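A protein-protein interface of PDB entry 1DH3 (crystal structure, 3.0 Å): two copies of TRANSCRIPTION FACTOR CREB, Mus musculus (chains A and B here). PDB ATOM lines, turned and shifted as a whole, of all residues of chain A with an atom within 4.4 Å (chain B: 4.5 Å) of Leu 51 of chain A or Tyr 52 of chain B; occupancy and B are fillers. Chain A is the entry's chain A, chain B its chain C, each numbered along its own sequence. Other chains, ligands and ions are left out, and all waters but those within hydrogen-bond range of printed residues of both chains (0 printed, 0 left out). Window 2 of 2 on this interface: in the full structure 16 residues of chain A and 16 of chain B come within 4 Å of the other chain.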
ATOM      1  N   ALA A  47     -12.696 -25.726 -12.378  1.00  0.00           N
ATOM      2  CA  ALA A  47     -11.243 -25.843 -12.222  1.00  0.00           C
ATOM      3  C   ALA A  47     -10.860 -25.351 -10.861  1.00  0.00           C
ATOM      4  O   ALA A  47     -10.890 -26.019  -9.860  1.00  0.00           O
ATOM      5  CB  ALA A  47     -10.664 -24.808 -13.067  1.00  0.00           C
ATOM      6  N   LEU A  48     -10.474 -24.109 -10.871  1.00  0.00           N
ATOM      7  CA  LEU A  48     -10.024 -23.414  -9.678  1.00  0.00           C
ATOM      8  C   LEU A  48     -10.622 -23.731  -8.283  1.00  0.00           C
ATOM      9  O   LEU A  48      -9.953 -23.463  -7.301  1.00  0.00           O
ATOM     10  CB  LEU A  48     -10.030 -21.890  -9.938  1.00  0.00           C
ATOM     11  CG  LEU A  48      -9.085 -21.486 -11.069  1.00  0.00           C
ATOM     12  CD1 LEU A  48      -8.216 -22.680 -11.531  1.00  0.00           C
ATOM     13  CD2 LEU A  48      -9.973 -21.119 -12.225  1.00  0.00           C
ATOM     14  N   LYS A  49     -11.841 -24.262  -8.149  1.00  0.00           N
ATOM     15  CA  LYS A  49     -12.332 -24.517  -6.773  1.00  0.00           C
ATOM     16  C   LYS A  49     -11.698 -25.769  -6.260  1.00  0.00           C
ATOM     17  O   LYS A  49     -11.341 -25.915  -5.035  1.00  0.00           O
ATOM     18  CB  LYS A  49     -13.841 -24.813  -6.695  1.00  0.00           C
ATOM     19  CG  LYS A  49     -14.162 -25.749  -5.496  1.00  0.00           C
ATOM     20  CD  LYS A  49     -15.053 -25.106  -4.373  1.00  0.00           C
ATOM     21  CE  LYS A  49     -16.304 -24.277  -4.886  1.00  0.00           C
ATOM     22  NZ  LYS A  49     -17.705 -24.596  -4.507  1.00  0.00           N
ATOM     23  N   ASP A  50     -11.573 -26.653  -7.224  1.00  0.00           N
ATOM     24  CA  ASP A  50     -10.984 -27.917  -6.921  1.00  0.00           C
ATOM     25  C   ASP A  50      -9.662 -27.766  -7.548  1.00  0.00           C
ATOM     26  O   ASP A  50      -9.393 -28.192  -8.690  1.00  0.00           O
ATOM     27  CB  ASP A  50     -11.784 -29.147  -7.356  1.00  0.00           C
ATOM     28  CG  ASP A  50     -12.291 -29.947  -6.109  1.00  0.00           C
ATOM     29  OD1 ASP A  50     -11.561 -30.875  -5.603  1.00  0.00           O
ATOM     30  OD2 ASP A  50     -13.407 -29.595  -5.586  1.00  0.00           O
ATOM     31  N   LEU A  51      -8.850 -27.099  -6.728  1.00  0.00           N
ATOM     32  CA  LEU A  51      -7.453 -26.724  -6.997  1.00  0.00           C
ATOM     33  C   LEU A  51      -7.322 -25.489  -6.019  1.00  0.00           C
ATOM     34  O   LEU A  51      -6.388 -24.594  -6.063  1.00  0.00           O
ATOM     35  CB  LEU A  51      -7.320 -26.260  -8.450  1.00  0.00           C
ATOM     36  CG  LEU A  51      -6.004 -25.472  -8.634  1.00  0.00           C
ATOM     37  CD1 LEU A  51      -4.860 -26.193  -8.108  1.00  0.00           C
ATOM     38  CD2 LEU A  51      -5.636 -24.724  -9.955  1.00  0.00           C
ATOM     39  N   TYR A  52      -8.330 -25.453  -5.162  1.00  0.00           N
ATOM     40  CA  TYR A  52      -8.409 -24.372  -4.169  1.00  0.00           C
ATOM     41  C   TYR A  52      -8.008 -24.919  -2.775  1.00  0.00           C
ATOM     42  O   TYR A  52      -8.277 -26.121  -2.436  1.00  0.00           O
ATOM     43  CB  TYR A  52      -9.881 -23.743  -4.107  1.00  0.00           C
ATOM     44  CG  TYR A  52     -10.039 -22.834  -2.871  1.00  0.00           C
ATOM     45  CD1 TYR A  52      -9.605 -21.519  -2.934  1.00  0.00           C
ATOM     46  CD2 TYR A  52     -10.600 -23.331  -1.693  1.00  0.00           C
ATOM     47  CE1 TYR A  52      -9.698 -20.730  -1.896  1.00  0.00           C
ATOM     48  CE2 TYR A  52     -10.701 -22.536  -0.629  1.00  0.00           C
ATOM     49  CZ  TYR A  52     -10.253 -21.250  -0.746  1.00  0.00           C
ATOM     50  OH  TYR A  52     -10.413 -20.445   0.354  1.00  0.00           O
ATOM     51  N   SER A  53      -7.390 -23.979  -2.030  1.00  0.00           N
ATOM     52  CA  SER A  53      -6.914 -24.236  -0.674  1.00  0.00           C
ATOM     53  C   SER A  53      -5.656 -25.099  -0.615  1.00  0.00           C
ATOM     54  O   SER A  53      -4.897 -25.085   0.374  1.00  0.00           O
ATOM     55  CB  SER A  53      -7.995 -24.810   0.292  1.00  0.00           C
ATOM     56  OG  SER A  53      -8.289 -23.818   1.259  1.00  0.00           O
ATOM     57  N   LEU B  48     -12.942 -16.035  -6.125  1.00  0.00           N
ATOM     58  CA  LEU B  48     -12.074 -17.206  -5.939  1.00  0.00           C
ATOM     59  C   LEU B  48     -10.698 -16.754  -6.385  1.00  0.00           C
ATOM     60  O   LEU B  48      -9.707 -17.055  -5.748  1.00  0.00           O
ATOM     61  CB  LEU B  48     -12.557 -18.499  -6.702  1.00  0.00           C
ATOM     62  CG  LEU B  48     -13.134 -19.621  -5.793  1.00  0.00           C
ATOM     63  CD1 LEU B  48     -14.414 -19.276  -4.995  1.00  0.00           C
ATOM     64  CD2 LEU B  48     -13.153 -21.015  -6.375  1.00  0.00           C
ATOM     65  N   LYS B  49     -10.725 -16.016  -7.465  1.00  0.00           N
ATOM     66  CA  LYS B  49      -9.476 -15.504  -8.007  1.00  0.00           C
ATOM     67  C   LYS B  49      -8.864 -14.710  -6.923  1.00  0.00           C
ATOM     68  O   LYS B  49      -7.671 -14.742  -6.730  1.00  0.00           O
ATOM     69  CB  LYS B  49      -9.764 -14.566  -9.139  1.00  0.00           C
ATOM     70  CG  LYS B  49      -8.610 -14.253 -10.162  1.00  0.00           C
ATOM     71  CD  LYS B  49      -8.571 -15.196 -11.319  1.00  0.00           C
ATOM     72  CE  LYS B  49      -9.135 -16.595 -11.079  1.00  0.00           C
ATOM     73  NZ  LYS B  49      -8.995 -17.327 -12.315  1.00  0.00           N
ATOM     74  N   ASP B  50      -9.722 -14.080  -6.159  1.00  0.00           N
ATOM     75  CA  ASP B  50      -9.404 -13.233  -5.046  1.00  0.00           C
ATOM     76  C   ASP B  50      -8.647 -13.912  -3.835  1.00  0.00           C
ATOM     77  O   ASP B  50      -7.909 -13.215  -3.116  1.00  0.00           O
ATOM     78  CB  ASP B  50     -10.651 -12.320  -4.840  1.00  0.00           C
ATOM     79  CG  ASP B  50     -10.562 -11.336  -3.700  1.00  0.00           C
ATOM     80  OD1 ASP B  50      -9.903 -11.647  -2.691  1.00  0.00           O
ATOM     81  OD2 ASP B  50     -11.342 -10.350  -3.683  1.00  0.00           O
ATOM     82  N   LEU B  51      -8.764 -15.224  -3.606  1.00  0.00           N
ATOM     83  CA  LEU B  51      -7.985 -15.792  -2.510  1.00  0.00           C
ATOM     84  C   LEU B  51      -7.026 -16.948  -3.110  1.00  0.00           C
ATOM     85  O   LEU B  51      -7.250 -18.094  -2.876  1.00  0.00           O
ATOM     86  CB  LEU B  51      -8.953 -16.053  -1.312  1.00  0.00           C
ATOM     87  CG  LEU B  51     -10.241 -16.887  -1.452  1.00  0.00           C
ATOM     88  CD1 LEU B  51     -11.385 -15.933  -1.362  1.00  0.00           C
ATOM     89  CD2 LEU B  51     -10.284 -17.623  -2.774  1.00  0.00           C
ATOM     90  N   TYR B  52      -5.927 -16.560  -3.857  1.00  0.00           N
ATOM     91  CA  TYR B  52      -4.888 -17.422  -4.589  1.00  0.00           C
ATOM     92  C   TYR B  52      -3.688 -18.184  -4.125  1.00  0.00           C
ATOM     93  O   TYR B  52      -2.696 -17.540  -3.732  1.00  0.00           O
ATOM     94  CB  TYR B  52      -4.362 -16.786  -5.953  1.00  0.00           C
ATOM     95  CG  TYR B  52      -4.428 -17.975  -6.892  1.00  0.00           C
ATOM     96  CD1 TYR B  52      -5.602 -18.718  -6.886  1.00  0.00           C
ATOM     97  CD2 TYR B  52      -3.362 -18.398  -7.656  1.00  0.00           C
ATOM     98  CE1 TYR B  52      -5.797 -19.787  -7.569  1.00  0.00           C
ATOM     99  CE2 TYR B  52      -3.598 -19.538  -8.538  1.00  0.00           C
ATOM    100  CZ  TYR B  52      -4.818 -20.195  -8.406  1.00  0.00           C
ATOM    101  OH  TYR B  52      -5.148 -21.266  -9.186  1.00  0.00           O
ATOM    102  N   SER B  53      -3.756 -19.526  -4.241  1.00  0.00           N
ATOM    103  CA  SER B  53      -2.680 -20.466  -3.809  1.00  0.00           C
ATOM    104  C   SER B  53      -2.979 -20.506  -2.223  1.00  0.00           C
ATOM    105  O   SER B  53      -2.407 -21.359  -1.515  1.00  0.00           O
ATOM    106  CB  SER B  53      -1.213 -20.004  -4.145  1.00  0.00           C
ATOM    107  OG  SER B  53      -0.561 -20.929  -5.019  1.00  0.00           O
ATOM    108  N   HIS B  54      -3.902 -19.615  -1.750  1.00  0.00           N
ATOM    109  CA  HIS B  54      -4.407 -19.417  -0.386  1.00  0.00           C
ATOM    110  C   HIS B  54      -5.043 -18.029  -0.127  1.00  0.00           C
ATOM    111  O   HIS B  54      -6.257 -18.110   0.064  1.00  0.00           O
ATOM    112  CB  HIS B  54      -3.471 -19.804   0.558  1.00  0.00           C
ATOM    113  CG  HIS B  54      -2.276 -18.940   0.487  1.00  0.00           C
ATOM    114  ND1 HIS B  54      -1.542 -18.732  -0.672  1.00  0.00           N
ATOM    115  CD2 HIS B  54      -1.737 -18.122   1.429  1.00  0.00           C
ATOM    116  CE1 HIS B  54      -0.563 -17.882  -0.421  1.00  0.00           C
ATOM    117  NE2 HIS B  54      -0.671 -17.475   0.842  1.00  0.00           N
ATOM    118  N   LYS B  55      -4.327 -16.760  -0.069  1.00  0.00           N
ATOM    119  CA  LYS B  55      -4.837 -15.182   0.126  1.00  0.00           C
ATOM    120  C   LYS B  55      -4.350 -14.745  -1.539  1.00  0.00           C
ATOM    121  O   LYS B  55      -3.338 -14.665  -1.813  1.00  0.00           O
ATOM    122  CB  LYS B  55      -4.052 -14.638   1.323  1.00  0.00           C
ATOM    123  CG  LYS B  55      -3.579 -13.221   1.175  1.00  0.00           C
ATOM    124  CD  LYS B  55      -4.284 -12.280   2.136  1.00  0.00           C
ATOM    125  CE  LYS B  55      -5.449 -11.553   1.477  1.00  0.00           C
ATOM    126  NZ  LYS B  55      -6.545 -12.447   1.076  1.00  0.00           N
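ND1 of His 54 of chain B is in hydrogen-bond range of O of Tyr 52 of chain B, 3.5 Å away.
Among the printed residues, pairs that only touch across the chains: Tyr 52 of chain A with Leu 51 of chain B, Leu 51 of chain A with Tyr 52 of chain B, Lys 49 of chain A with Leu 48 of chain B and Leu 48 of chain A with Lys 49 of chain B.
Leu 51 of chain A touches one residue of chain B. Printed residues of chain A within 4 Å of Lys 49 of chain B: Leu 48. Of the printed residues of chain A, Leu 51 of chain B touches Tyr 52 (3.3 Å). Tyr 52 of chain B touches just one residue of chain A: Leu 51. The nearest printed residue of chain B that does not touch Leu 51 of chain A is Ser 53 of chain B (6.0 Å). The nearest printed residue of chain A that does not touch Lys 49 of chain B is Tyr 52 of chain A (7.2 Å).
Of the 8 printed residues of chain B, 4 touch a printed residue of chain A. Hydrophobic or aromatic side chains of chain B within 4 Å of the printed part of chain A: Leu 48, Leu 51 and Tyr 52. Hydrophobic or aromatic side chains of chain A within 4 Å of the printed part of chain B: Leu 48, Leu 51 and Tyr 52. Among the printed residues, 4 pairs touch across the chains. Among the printed residues, no Asp or Glu carboxylate lies within 4 Å of a Lys or Arg side-chain nitrogen of the other chain.
Leu 48 of chain A touches Lys 49 of chain B, and with the chains exchanged Lys 49 of chain A touches Leu 48 of chain B. Leu 51 of chain A touches Tyr 52 of chain B, and with the chains exchanged Tyr 52 of chain A touches Leu 51 of chain B. Of the 4 pairs that touch across the chains among the printed residues, 4 have their exchanged pair printed and touching as well.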
